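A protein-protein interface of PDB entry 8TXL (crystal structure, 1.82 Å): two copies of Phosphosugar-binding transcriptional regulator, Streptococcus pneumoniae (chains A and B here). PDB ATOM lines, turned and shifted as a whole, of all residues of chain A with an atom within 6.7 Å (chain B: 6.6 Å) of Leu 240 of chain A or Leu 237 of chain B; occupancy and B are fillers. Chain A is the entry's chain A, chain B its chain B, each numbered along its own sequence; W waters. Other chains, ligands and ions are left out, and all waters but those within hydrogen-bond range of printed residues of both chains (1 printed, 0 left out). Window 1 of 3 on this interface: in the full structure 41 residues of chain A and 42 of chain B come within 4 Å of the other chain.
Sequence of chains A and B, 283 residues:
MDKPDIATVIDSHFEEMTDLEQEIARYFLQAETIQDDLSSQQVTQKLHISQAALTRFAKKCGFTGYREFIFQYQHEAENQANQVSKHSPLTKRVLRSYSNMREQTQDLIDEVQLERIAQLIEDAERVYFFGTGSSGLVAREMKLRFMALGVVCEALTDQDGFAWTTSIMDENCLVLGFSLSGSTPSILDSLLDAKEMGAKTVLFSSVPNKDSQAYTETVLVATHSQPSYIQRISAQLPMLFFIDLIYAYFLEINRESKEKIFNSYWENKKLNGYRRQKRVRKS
The side-chain hydroxyl of Tyr 98 of chain A sits at hydrogen-bond distance from the backbone carbonyl oxygen of Leu 240 of chain B, 3.3 Å away. The side-chain hydroxyl (OH) of Tyr 98 of chain A lies within hydrogen-bond range of the backbone NH (N) of Phe 241 of chain B, 3.4 Å away. OG of Ser 234 of chain B lies within hydrogen-bond range of OE2 of Glu 141 of chain A, 2.9 Å away. The side-chain carboxylate of Glu 141 of chain A sits close to the side-chain amide oxygen of Gln 236 of chain B (3.1 Å). The side-chain carboxylate of Glu 141 of chain B sits close to the side-chain hydroxyl of Ser 234 of chain A (3.3 Å). OE2 of Glu 141 of chain B is in hydrogen-bond range of N of Ala 235 of chain A, 3.5 Å away. The side-chain amide oxygen (OE1) of Gln 236 of chain A sits close to the side-chain carboxylate (OE1) of Glu 141 of chain B (3.0 Å). The side-chain amide oxygen of Gln 236 of chain A sits at hydrogen-bond distance from the side-chain amide nitrogen of Gln 236 of chain B. The side-chain hydroxyl of Tyr 98 of chain B lies within hydrogen-bond range of the side-chain carboxylate of Asp 244 of chain A (2.6 Å). The side-chain carboxylate (OD2) of Asp 244 of chain A is in hydrogen-bond range of the backbone NH (N) of Ser 234 of chain B, 3.0 Å away.
The side-chain hydroxyl (OG) of Ser 234 of chain A sits at hydrogen-bond distance from the backbone NH (N) of Gln 236 of chain A, 3.1 Å away.
Arg 145 of chain A touches Ile 233 of chain B. Ser 234 of chain B touches Arg 145 of chain A. Asp 244 of chain A touches Val 94 of chain B (CB to CG1, 3.9 Å). Leu 245 of chain A touches Val 94 of chain B (CD2 to CG1, 3.9 Å).
Leu 240 of chain A touches just these residues of chain B: Tyr 98 (3.2 Å), Leu 237 (3.6 Å) and Leu 240 (3.7 Å). Leu 237 of chain B touches just one residue of chain A: Leu 240 (3.6 Å). Of the printed residues of chain B, Asp 244 of chain A touches Val 94, Tyr 98, Ile 233 and Ser 234. Met 142 of chain A touches none of the printed residues of chain B. Pro 238 of chain B touches none of the printed residues of chain A. The nearest residue of chain A that does not touch Leu 237 of chain B is Leu 237 of chain A (4.2 Å). The nearest printed residue of chain A that does not touch Leu 240 of chain B is Ser 234 of chain A (4.1 Å).
Of the 18 printed residues of chain B, 9 touch a printed residue of chain A. Of the 18 printed residues of chain A, 11 touch a printed residue of chain B. Hydrophobic or aromatic side chains of chain A that line the printed part of chain B: Tyr 98, Leu 137, Leu 240, Phe 241 and Leu 245. Along chain A the printed residues that touch a printed residue of chain B span positions 98 to 245.
Glu 141 of chain A touches Gln 236 of chain B, and with the chains exchanged Gln 236 of chain A touches Glu 141 of chain B.
Water W1 lies within hydrogen-bond range of OE2 of Glu 141 of chain A (2.7 Å) and N of Ala 235 of chain B (2.8 Å).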
ATOM      1  N   TYR A  98     -19.497 -26.612   9.712  1.00  0.00           N
ATOM      2  CA  TYR A  98     -19.187 -26.289  11.099  1.00  0.00           C
ATOM      3  C   TYR A  98     -17.696 -26.356  11.379  1.00  0.00           C
ATOM      4  O   TYR A  98     -17.146 -25.486  12.060  1.00  0.00           O
ATOM      5  CB  TYR A  98     -19.921 -27.253  12.027  1.00  0.00           C
ATOM      6  CG  TYR A  98     -21.326 -26.790  12.311  1.00  0.00           C
ATOM      7  CD1 TYR A  98     -22.367 -27.056  11.423  1.00  0.00           C
ATOM      8  CD2 TYR A  98     -21.607 -26.041  13.437  1.00  0.00           C
ATOM      9  CE1 TYR A  98     -23.640 -26.619  11.690  1.00  0.00           C
ATOM     10  CE2 TYR A  98     -22.852 -25.603  13.698  1.00  0.00           C
ATOM     11  CZ  TYR A  98     -23.861 -25.883  12.849  1.00  0.00           C
ATOM     12  OH  TYR A  98     -25.108 -25.415  13.168  1.00  0.00           O
ATOM     13  N   LEU A 137     -30.652 -11.806  16.815  1.00  0.00           N
ATOM     14  CA  LEU A 137     -30.646 -12.974  17.671  1.00  0.00           C
ATOM     15  C   LEU A 137     -29.320 -13.118  18.397  1.00  0.00           C
ATOM     16  O   LEU A 137     -29.290 -13.455  19.589  1.00  0.00           O
ATOM     17  CB  LEU A 137     -30.963 -14.219  16.848  1.00  0.00           C
ATOM     18  CG  LEU A 137     -32.293 -14.221  16.072  1.00  0.00           C
ATOM     19  CD1 LEU A 137     -32.310 -15.547  15.317  1.00  0.00           C
ATOM     20  CD2 LEU A 137     -33.495 -14.067  16.991  1.00  0.00           C
ATOM     21  N   VAL A 138     -28.214 -12.841  17.695  1.00  0.00           N
ATOM     22  CA  VAL A 138     -26.899 -12.816  18.326  1.00  0.00           C
ATOM     23  C   VAL A 138     -26.868 -11.781  19.454  1.00  0.00           C
ATOM     24  O   VAL A 138     -26.356 -12.048  20.558  1.00  0.00           O
ATOM     25  CB  VAL A 138     -25.829 -12.524  17.248  1.00  0.00           C
ATOM     26  CG1 VAL A 138     -24.490 -12.132  17.875  1.00  0.00           C
ATOM     27  CG2 VAL A 138     -25.702 -13.732  16.308  1.00  0.00           C
ATOM     28  N   GLU A 141     -28.701 -13.078  22.349  1.00  0.00           N
ATOM     29  CA  GLU A 141     -27.939 -14.139  22.974  1.00  0.00           C
ATOM     30  C   GLU A 141     -26.851 -13.559  23.858  1.00  0.00           C
ATOM     31  O   GLU A 141     -26.607 -14.050  24.969  1.00  0.00           O
ATOM     32  CB  GLU A 141     -27.331 -15.040  21.894  1.00  0.00           C
ATOM     33  CG  GLU A 141     -26.308 -15.982  22.402  1.00  0.00           C
ATOM     34  CD  GLU A 141     -26.937 -17.225  23.012  1.00  0.00           C
ATOM     35  OE1 GLU A 141     -28.179 -17.355  23.069  1.00  0.00           O
ATOM     36  OE2 GLU A 141     -26.184 -18.074  23.460  1.00  0.00           O
ATOM     37  N   MET A 142     -26.146 -12.537  23.353  1.00  0.00           N
ATOM     38  CA  MET A 142     -25.070 -11.986  24.162  1.00  0.00           C
ATOM     39  C   MET A 142     -25.593 -11.421  25.466  1.00  0.00           C
ATOM     40  O   MET A 142     -24.947 -11.539  26.501  1.00  0.00           O
ATOM     41  CB  MET A 142     -24.306 -10.905  23.410  1.00  0.00           C
ATOM     42  CG  MET A 142     -22.852 -10.819  23.891  1.00  0.00           C
ATOM     43  SD  MET A 142     -21.830  -9.851  22.749  1.00  0.00           S
ATOM     44  CE  MET A 142     -20.269  -9.943  23.593  1.00  0.00           C
ATOM     45  N   ARG A 145     -26.015 -14.049  28.040  1.00  0.00           N
ATOM     46  CA  ARG A 145     -24.781 -14.578  28.630  1.00  0.00           C
ATOM     47  C   ARG A 145     -24.200 -13.596  29.640  1.00  0.00           C
ATOM     48  O   ARG A 145     -23.761 -13.987  30.735  1.00  0.00           O
ATOM     49  CB  ARG A 145     -23.723 -14.858  27.561  1.00  0.00           C
ATOM     50  CG  ARG A 145     -24.111 -15.741  26.368  1.00  0.00           C
ATOM     51  CD  ARG A 145     -24.476 -17.127  26.771  1.00  0.00           C
ATOM     52  NE  ARG A 145     -23.545 -17.662  27.754  1.00  0.00           N
ATOM     53  CZ  ARG A 145     -22.500 -18.427  27.459  1.00  0.00           C
ATOM     54  NH1 ARG A 145     -22.048 -18.541  26.216  1.00  0.00           N
ATOM     55  NH2 ARG A 145     -21.870 -19.063  28.444  1.00  0.00           N
ATOM     56  N   SER A 234     -26.127 -21.910   9.927  1.00  0.00           N
ATOM     57  CA  SER A 234     -26.698 -20.794  10.671  1.00  0.00           C
ATOM     58  C   SER A 234     -25.880 -19.525  10.486  1.00  0.00           C
ATOM     59  O   SER A 234     -24.649 -19.534  10.586  1.00  0.00           O
ATOM     60  CB  SER A 234     -26.756 -21.147  12.165  1.00  0.00           C
ATOM     61  OG  SER A 234     -27.051 -19.987  12.929  1.00  0.00           O
ATOM     62  N   ALA A 235     -26.568 -18.440  10.194  1.00  0.00           N
ATOM     63  CA  ALA A 235     -25.914 -17.141  10.093  1.00  0.00           C
ATOM     64  C   ALA A 235     -25.448 -16.618  11.445  1.00  0.00           C
ATOM     65  O   ALA A 235     -24.604 -15.729  11.485  1.00  0.00           O
ATOM     66  CB  ALA A 235     -26.864 -16.103   9.477  1.00  0.00           C
ATOM     67  N   GLN A 236     -25.970 -17.142  12.564  1.00  0.00           N
ATOM     68  CA  GLN A 236     -25.459 -16.710  13.853  1.00  0.00           C
ATOM     69  C   GLN A 236     -24.048 -17.198  14.128  1.00  0.00           C
ATOM     70  O   GLN A 236     -23.333 -16.611  14.954  1.00  0.00           O
ATOM     71  CB  GLN A 236     -26.346 -17.249  14.969  1.00  0.00           C
ATOM     72  CG  GLN A 236     -27.755 -16.786  14.893  1.00  0.00           C
ATOM     73  CD  GLN A 236     -28.482 -17.279  16.132  1.00  0.00           C
ATOM     74  OE1 GLN A 236     -29.365 -18.154  16.058  1.00  0.00           O
ATOM     75  NE2 GLN A 236     -28.100 -16.741  17.279  1.00  0.00           N
ATOM     76  N   LEU A 237     -23.665 -18.317  13.541  1.00  0.00           N
ATOM     77  CA  LEU A 237     -22.501 -19.024  14.066  1.00  0.00           C
ATOM     78  C   LEU A 237     -21.207 -18.216  14.072  1.00  0.00           C
ATOM     79  O   LEU A 237     -20.446 -18.326  15.057  1.00  0.00           O
ATOM     80  CB  LEU A 237     -22.274 -20.322  13.268  1.00  0.00           C
ATOM     81  CG  LEU A 237     -21.246 -21.246  13.909  1.00  0.00           C
ATOM     82  CD1 LEU A 237     -21.571 -21.587  15.396  1.00  0.00           C
ATOM     83  CD2 LEU A 237     -21.093 -22.579  13.127  1.00  0.00           C
ATOM     84  N   PRO A 238     -20.829 -17.513  12.995  1.00  0.00           N
ATOM     85  CA  PRO A 238     -19.587 -16.719  13.049  1.00  0.00           C
ATOM     86  C   PRO A 238     -19.534 -15.832  14.289  1.00  0.00           C
ATOM     87  O   PRO A 238     -18.480 -15.690  14.922  1.00  0.00           O
ATOM     88  CB  PRO A 238     -19.637 -15.905  11.737  1.00  0.00           C
ATOM     89  CG  PRO A 238     -20.556 -16.695  10.816  1.00  0.00           C
ATOM     90  CD  PRO A 238     -21.590 -17.288  11.752  1.00  0.00           C
ATOM     91  N   MET A 239     -20.674 -15.253  14.664  1.00  0.00           N
ATOM     92  CA  MET A 239     -20.707 -14.367  15.812  1.00  0.00           C
ATOM     93  C   MET A 239     -20.676 -15.147  17.129  1.00  0.00           C
ATOM     94  O   MET A 239     -20.015 -14.727  18.096  1.00  0.00           O
ATOM     95  CB  MET A 239     -21.944 -13.475  15.759  1.00  0.00           C
ATOM     96  CG  MET A 239     -22.184 -12.757  14.469  1.00  0.00           C
ATOM     97  SD  MET A 239     -20.805 -11.649  14.240  1.00  0.00           S
ATOM     98  CE  MET A 239     -21.414 -10.697  12.790  1.00  0.00           C
ATOM     99  N   LEU A 240     -21.374 -16.291  17.188  1.00  0.00           N
ATOM    100  CA  LEU A 240     -21.421 -17.016  18.448  1.00  0.00           C
ATOM    101  C   LEU A 240     -20.025 -17.404  18.888  1.00  0.00           C
ATOM    102  O   LEU A 240     -19.724 -17.398  20.085  1.00  0.00           O
ATOM    103  CB  LEU A 240     -22.314 -18.241  18.337  1.00  0.00           C
ATOM    104  CG  LEU A 240     -23.773 -17.947  18.060  1.00  0.00           C
ATOM    105  CD1 LEU A 240     -24.518 -19.246  17.818  1.00  0.00           C
ATOM    106  CD2 LEU A 240     -24.429 -17.183  19.163  1.00  0.00           C
ATOM    107  N   PHE A 241     -19.151 -17.777  17.940  1.00  0.00           N
ATOM    108  CA  PHE A 241     -17.779 -18.100  18.296  1.00  0.00           C
ATOM    109  C   PHE A 241     -17.147 -16.974  19.088  1.00  0.00           C
ATOM    110  O   PHE A 241     -16.519 -17.200  20.127  1.00  0.00           O
ATOM    111  CB  PHE A 241     -16.942 -18.358  17.028  1.00  0.00           C
ATOM    112  CG  PHE A 241     -16.965 -19.764  16.565  1.00  0.00           C
ATOM    113  CD1 PHE A 241     -16.178 -20.691  17.194  1.00  0.00           C
ATOM    114  CD2 PHE A 241     -17.737 -20.167  15.479  1.00  0.00           C
ATOM    115  CE1 PHE A 241     -16.167 -22.019  16.805  1.00  0.00           C
ATOM    116  CE2 PHE A 241     -17.693 -21.555  15.066  1.00  0.00           C
ATOM    117  CZ  PHE A 241     -16.921 -22.429  15.750  1.00  0.00           C
ATOM    118  N   PHE A 242     -17.273 -15.738  18.583  1.00  0.00           N
ATOM    119  CA  PHE A 242     -16.655 -14.589  19.248  1.00  0.00           C
ATOM    120  C   PHE A 242     -17.355 -14.184  20.528  1.00  0.00           C
ATOM    121  O   PHE A 242     -16.675 -13.796  21.489  1.00  0.00           O
ATOM    122  CB  PHE A 242     -16.557 -13.436  18.239  1.00  0.00           C
ATOM    123  CG  PHE A 242     -15.392 -13.620  17.283  1.00  0.00           C
ATOM    124  CD1 PHE A 242     -15.520 -14.388  16.131  1.00  0.00           C
ATOM    125  CD2 PHE A 242     -14.133 -13.127  17.608  1.00  0.00           C
ATOM    126  CE1 PHE A 242     -14.413 -14.606  15.284  1.00  0.00           C
ATOM    127  CE2 PHE A 242     -13.049 -13.342  16.793  1.00  0.00           C
ATOM    128  CZ  PHE A 242     -13.189 -14.089  15.620  1.00  0.00           C
ATOM    129  N   ILE A 243     -18.685 -14.324  20.595  1.00  0.00           N
ATOM    130  CA  ILE A 243     -19.354 -14.152  21.885  1.00  0.00           C
ATOM    131  C   ILE A 243     -18.754 -15.087  22.918  1.00  0.00           C
ATOM    132  O   ILE A 243     -18.492 -14.696  24.058  1.00  0.00           O
ATOM    133  CB  ILE A 243     -20.880 -14.357  21.745  1.00  0.00           C
ATOM    134  CG1 ILE A 243     -21.498 -13.161  21.027  1.00  0.00           C
ATOM    135  CG2 ILE A 243     -21.539 -14.571  23.126  1.00  0.00           C
ATOM    136  CD1 ILE A 243     -22.935 -13.431  20.590  1.00  0.00           C
ATOM    137  N   ASP A 244     -18.551 -16.362  22.571  1.00  0.00           N
ATOM    138  CA  ASP A 244     -18.059 -17.297  23.570  1.00  0.00           C
ATOM    139  C   ASP A 244     -16.615 -17.005  23.962  1.00  0.00           C
ATOM    140  O   ASP A 244     -16.233 -17.192  25.126  1.00  0.00           O
ATOM    141  CB  ASP A 244     -18.185 -18.733  23.042  1.00  0.00           C
ATOM    142  CG  ASP A 244     -19.542 -19.352  23.397  1.00  0.00           C
ATOM    143  OD1 ASP A 244     -19.918 -19.221  24.578  1.00  0.00           O
ATOM    144  OD2 ASP A 244     -20.190 -20.012  22.534  1.00  0.00           O
ATOM    145  N   LEU A 245     -15.801 -16.555  22.997  1.00  0.00           N
ATOM    146  CA  LEU A 245     -14.422 -16.213  23.293  1.00  0.00           C
ATOM    147  C   LEU A 245     -14.334 -15.013  24.228  1.00  0.00           C
ATOM    148  O   LEU A 245     -13.690 -15.065  25.281  1.00  0.00           O
ATOM    149  CB  LEU A 245     -13.688 -15.934  21.978  1.00  0.00           C
ATOM    150  CG  LEU A 245     -13.330 -17.221  21.191  1.00  0.00           C
ATOM    151  CD1 LEU A 245     -12.895 -16.875  19.759  1.00  0.00           C
ATOM    152  CD2 LEU A 245     -12.255 -18.003  21.874  1.00  0.00           C
ATOM    153  N   VAL B  94     -12.407 -22.928  24.840  1.00  0.00           N
ATOM    154  CA  VAL B  94     -13.606 -22.592  24.075  1.00  0.00           C
ATOM    155  C   VAL B  94     -13.629 -23.333  22.748  1.00  0.00           C
ATOM    156  O   VAL B  94     -14.661 -23.866  22.329  1.00  0.00           O
ATOM    157  CB  VAL B  94     -13.692 -21.068  23.868  1.00  0.00           C
ATOM    158  CG1 VAL B  94     -14.864 -20.723  22.942  1.00  0.00           C
ATOM    159  CG2 VAL B  94     -13.808 -20.357  25.195  1.00  0.00           C
ATOM    160  N   TYR B  98     -16.307 -26.350  21.171  1.00  0.00           N
ATOM    161  CA  TYR B  98     -16.983 -26.447  19.891  1.00  0.00           C
ATOM    162  C   TYR B  98     -16.607 -27.749  19.165  1.00  0.00           C
ATOM    163  O   TYR B  98     -17.482 -28.425  18.593  1.00  0.00           O
ATOM    164  CB  TYR B  98     -16.635 -25.243  19.009  1.00  0.00           C
ATOM    165  CG  TYR B  98     -17.465 -24.000  19.302  1.00  0.00           C
ATOM    166  CD1 TYR B  98     -17.163 -23.175  20.353  1.00  0.00           C
ATOM    167  CD2 TYR B  98     -18.501 -23.654  18.466  1.00  0.00           C
ATOM    168  CE1 TYR B  98     -17.919 -22.000  20.592  1.00  0.00           C
ATOM    169  CE2 TYR B  98     -19.280 -22.498  18.687  1.00  0.00           C
ATOM    170  CZ  TYR B  98     -18.976 -21.689  19.769  1.00  0.00           C
ATOM    171  OH  TYR B  98     -19.743 -20.556  20.025  1.00  0.00           O
ATOM    172  N   MET B 101     -18.351 -30.654  20.749  1.00  0.00           N
ATOM    173  CA  MET B 101     -19.773 -30.754  20.431  1.00  0.00           C
ATOM    174  C   MET B 101     -20.023 -31.221  19.012  1.00  0.00           C
ATOM    175  O   MET B 101     -20.996 -31.921  18.768  1.00  0.00           O
ATOM    176  CB  MET B 101     -20.481 -29.421  20.656  1.00  0.00           C
ATOM    177  CG  MET B 101     -21.975 -29.564  20.660  1.00  0.00           C
ATOM    178  SD  MET B 101     -22.737 -27.988  21.124  1.00  0.00           S
ATOM    179  CE  MET B 101     -22.058 -27.780  22.750  1.00  0.00           C
ATOM    180  N   THR B 105     -22.101 -34.606  18.332  1.00  0.00           N
ATOM    181  CA  THR B 105     -23.229 -34.504  17.420  1.00  0.00           C
ATOM    182  C   THR B 105     -23.136 -35.553  16.319  1.00  0.00           C
ATOM    183  O   THR B 105     -24.121 -36.216  15.967  1.00  0.00           O
ATOM    184  CB  THR B 105     -23.246 -33.105  16.792  1.00  0.00           C
ATOM    185  OG1 THR B 105     -23.537 -32.141  17.821  1.00  0.00           O
ATOM    186  CG2 THR B 105     -24.273 -33.005  15.696  1.00  0.00           C
ATOM    187  N   VAL B 138     -33.121 -20.100  18.775  1.00  0.00           N
ATOM    188  CA  VAL B 138     -33.014 -21.153  17.767  1.00  0.00           C
ATOM    189  C   VAL B 138     -34.324 -21.240  16.995  1.00  0.00           C
ATOM    190  O   VAL B 138     -34.340 -21.241  15.764  1.00  0.00           O
ATOM    191  CB  VAL B 138     -32.641 -22.485  18.430  1.00  0.00           C
ATOM    192  CG1 VAL B 138     -32.783 -23.630  17.441  1.00  0.00           C
ATOM    193  CG2 VAL B 138     -31.208 -22.415  18.945  1.00  0.00           C
ATOM    194  N   GLU B 141     -34.636 -18.344  14.589  1.00  0.00           N
ATOM    195  CA  GLU B 141     -33.768 -18.529  13.425  1.00  0.00           C
ATOM    196  C   GLU B 141     -34.370 -19.553  12.456  1.00  0.00           C
ATOM    197  O   GLU B 141     -34.527 -19.278  11.267  1.00  0.00           O
ATOM    198  CB  GLU B 141     -32.367 -18.972  13.840  1.00  0.00           C
ATOM    199  CG  GLU B 141     -31.538 -19.418  12.631  1.00  0.00           C
ATOM    200  CD  GLU B 141     -30.064 -19.069  12.691  1.00  0.00           C
ATOM    201  OE1 GLU B 141     -29.330 -19.661  13.506  1.00  0.00           O
ATOM    202  OE2 GLU B 141     -29.615 -18.234  11.872  1.00  0.00           O
ATOM    203  N   LEU B 180     -33.385 -27.979  25.844  1.00  0.00           N
ATOM    204  CA  LEU B 180     -32.048 -28.560  25.977  1.00  0.00           C
ATOM    205  C   LEU B 180     -31.959 -29.414  27.228  1.00  0.00           C
ATOM    206  O   LEU B 180     -31.294 -30.457  27.230  1.00  0.00           O
ATOM    207  CB  LEU B 180     -30.979 -27.461  25.997  1.00  0.00           C
ATOM    208  CG  LEU B 180     -29.501 -27.836  25.790  1.00  0.00           C
ATOM    209  CD1 LEU B 180     -29.372 -28.610  24.483  1.00  0.00           C
ATOM    210  CD2 LEU B 180     -28.555 -26.613  25.792  1.00  0.00           C
ATOM    211  N   HIS B 224     -23.271 -30.575  26.715  1.00  0.00           N
ATOM    212  CA  HIS B 224     -22.090 -29.720  26.753  1.00  0.00           C
ATOM    213  C   HIS B 224     -20.876 -30.419  27.396  1.00  0.00           C
ATOM    214  O   HIS B 224     -21.008 -31.290  28.253  1.00  0.00           O
ATOM    215  CB  HIS B 224     -22.376 -28.410  27.502  1.00  0.00           C
ATOM    216  CG  HIS B 224     -23.228 -27.443  26.725  1.00  0.00           C
ATOM    217  ND1 HIS B 224     -22.718 -26.299  26.156  1.00  0.00           N
ATOM    218  CD2 HIS B 224     -24.536 -27.482  26.386  1.00  0.00           C
ATOM    219  CE1 HIS B 224     -23.687 -25.658  25.505  1.00  0.00           C
ATOM    220  NE2 HIS B 224     -24.801 -26.352  25.637  1.00  0.00           N
ATOM    221  N   ILE B 233     -20.244 -23.116  26.646  1.00  0.00           N
ATOM    222  CA  ILE B 233     -20.421 -22.323  25.433  1.00  0.00           C
ATOM    223  C   ILE B 233     -21.910 -22.255  25.144  1.00  0.00           C
ATOM    224  O   ILE B 233     -22.745 -22.805  25.898  1.00  0.00           O
ATOM    225  CB  ILE B 233     -19.651 -22.884  24.214  1.00  0.00           C
ATOM    226  CG1 ILE B 233     -20.017 -24.338  23.935  1.00  0.00           C
ATOM    227  CG2 ILE B 233     -18.130 -22.772  24.429  1.00  0.00           C
ATOM    228  CD1 ILE B 233     -19.534 -24.891  22.470  1.00  0.00           C
ATOM    229  N   SER B 234     -22.264 -21.616  24.033  1.00  0.00           N
ATOM    230  CA  SER B 234     -23.646 -21.186  23.849  1.00  0.00           C
ATOM    231  C   SER B 234     -24.640 -22.342  23.955  1.00  0.00           C
ATOM    232  O   SER B 234     -24.422 -23.425  23.407  1.00  0.00           O
ATOM    233  CB  SER B 234     -23.810 -20.508  22.488  1.00  0.00           C
ATOM    234  OG  SER B 234     -25.178 -20.452  22.128  1.00  0.00           O
ATOM    235  N   ALA B 235     -25.733 -22.107  24.697  1.00  0.00           N
ATOM    236  CA  ALA B 235     -26.802 -23.108  24.810  1.00  0.00           C
ATOM    237  C   ALA B 235     -27.532 -23.343  23.492  1.00  0.00           C
ATOM    238  O   ALA B 235     -28.260 -24.326  23.373  1.00  0.00           O
ATOM    239  CB  ALA B 235     -27.816 -22.670  25.893  1.00  0.00           C
ATOM    240  N   GLN B 236     -27.414 -22.446  22.504  1.00  0.00           N
ATOM    241  CA  GLN B 236     -28.070 -22.713  21.220  1.00  0.00           C
ATOM    242  C   GLN B 236     -27.392 -23.874  20.458  1.00  0.00           C
ATOM    243  O   GLN B 236     -28.010 -24.476  19.575  1.00  0.00           O
ATOM    244  CB  GLN B 236     -27.989 -21.499  20.275  1.00  0.00           C
ATOM    245  CG  GLN B 236     -28.660 -20.181  20.787  1.00  0.00           C
ATOM    246  CD  GLN B 236     -28.724 -19.127  19.735  1.00  0.00           C
ATOM    247  OE1 GLN B 236     -28.399 -17.982  19.991  1.00  0.00           O
ATOM    248  NE2 GLN B 236     -29.233 -19.482  18.558  1.00  0.00           N
ATOM    249  N   LEU B 237     -26.123 -24.078  20.716  1.00  0.00           N
ATOM    250  CA  LEU B 237     -25.266 -24.810  19.749  1.00  0.00           C
ATOM    251  C   LEU B 237     -25.696 -26.237  19.535  1.00  0.00           C
ATOM    252  O   LEU B 237     -25.847 -26.636  18.357  1.00  0.00           O
ATOM    253  CB  LEU B 237     -23.823 -24.731  20.224  1.00  0.00           C
ATOM    254  CG  LEU B 237     -22.897 -23.840  19.407  1.00  0.00           C
ATOM    255  CD1 LEU B 237     -22.586 -24.634  18.114  1.00  0.00           C
ATOM    256  CD2 LEU B 237     -23.394 -22.469  19.108  1.00  0.00           C
ATOM    257  N   PRO B 238     -26.027 -27.029  20.552  1.00  0.00           N
ATOM    258  CA  PRO B 238     -26.496 -28.403  20.303  1.00  0.00           C
ATOM    259  C   PRO B 238     -27.682 -28.447  19.370  1.00  0.00           C
ATOM    260  O   PRO B 238     -27.767 -29.313  18.489  1.00  0.00           O
ATOM    261  CB  PRO B 238     -26.859 -28.917  21.709  1.00  0.00           C
ATOM    262  CG  PRO B 238     -26.032 -28.074  22.605  1.00  0.00           C
ATOM    263  CD  PRO B 238     -26.044 -26.709  21.986  1.00  0.00           C
ATOM    264  N   MET B 239     -28.578 -27.478  19.498  1.00  0.00           N
ATOM    265  CA  MET B 239     -29.750 -27.437  18.646  1.00  0.00           C
ATOM    266  C   MET B 239     -29.389 -26.992  17.247  1.00  0.00           C
ATOM    267  O   MET B 239     -29.950 -27.489  16.273  1.00  0.00           O
ATOM    268  CB  MET B 239     -30.810 -26.488  19.216  1.00  0.00           C
ATOM    269  CG  MET B 239     -31.093 -26.698  20.677  1.00  0.00           C
ATOM    270  SD  MET B 239     -32.015 -28.237  20.825  1.00  0.00           S
ATOM    271  CE  MET B 239     -32.491 -28.126  22.581  1.00  0.00           C
ATOM    272  N   LEU B 240     -28.519 -25.989  17.131  1.00  0.00           N
ATOM    273  CA  LEU B 240     -28.256 -25.420  15.812  1.00  0.00           C
ATOM    274  C   LEU B 240     -27.736 -26.480  14.845  1.00  0.00           C
ATOM    275  O   LEU B 240     -28.132 -26.500  13.669  1.00  0.00           O
ATOM    276  CB  LEU B 240     -27.278 -24.242  15.944  1.00  0.00           C
ATOM    277  CG  LEU B 240     -27.864 -22.932  16.484  1.00  0.00           C
ATOM    278  CD1 LEU B 240     -26.653 -21.961  16.628  1.00  0.00           C
ATOM    279  CD2 LEU B 240     -28.973 -22.360  15.629  1.00  0.00           C
ATOM    280  N   PHE B 241     -26.881 -27.389  15.331  1.00  0.00           N
ATOM    281  CA  PHE B 241     -26.386 -28.482  14.507  1.00  0.00           C
ATOM    282  C   PHE B 241     -27.521 -29.252  13.844  1.00  0.00           C
ATOM    283  O   PHE B 241     -27.498 -29.504  12.633  1.00  0.00           O
ATOM    284  CB  PHE B 241     -25.574 -29.449  15.346  1.00  0.00           C
ATOM    285  CG  PHE B 241     -24.152 -29.079  15.521  1.00  0.00           C
ATOM    286  CD1 PHE B 241     -23.224 -29.363  14.524  1.00  0.00           C
ATOM    287  CD2 PHE B 241     -23.699 -28.529  16.696  1.00  0.00           C
ATOM    288  CE1 PHE B 241     -21.907 -29.068  14.682  1.00  0.00           C
ATOM    289  CE2 PHE B 241     -22.347 -28.257  16.862  1.00  0.00           C
ATOM    290  CZ  PHE B 241     -21.466 -28.534  15.844  1.00  0.00           C
ATOM    291  N   PHE B 242     -28.535 -29.659  14.639  1.00  0.00           N
ATOM    292  CA  PHE B 242     -29.586 -30.509  14.101  1.00  0.00           C
ATOM    293  C   PHE B 242     -30.538 -29.712  13.268  1.00  0.00           C
ATOM    294  O   PHE B 242     -31.014 -30.224  12.248  1.00  0.00           O
ATOM    295  CB  PHE B 242     -30.254 -31.267  15.269  1.00  0.00           C
ATOM    296  CG  PHE B 242     -29.440 -32.446  15.715  1.00  0.00           C
ATOM    297  CD1 PHE B 242     -29.555 -33.644  15.033  1.00  0.00           C
ATOM    298  CD2 PHE B 242     -28.513 -32.339  16.739  1.00  0.00           C
ATOM    299  CE1 PHE B 242     -28.772 -34.774  15.404  1.00  0.00           C
ATOM    300  CE2 PHE B 242     -27.723 -33.439  17.106  1.00  0.00           C
ATOM    301  CZ  PHE B 242     -27.845 -34.648  16.422  1.00  0.00           C
HETATM  302  O   HOH W   1     -26.345 -19.591  25.688  1.00  0.00           O
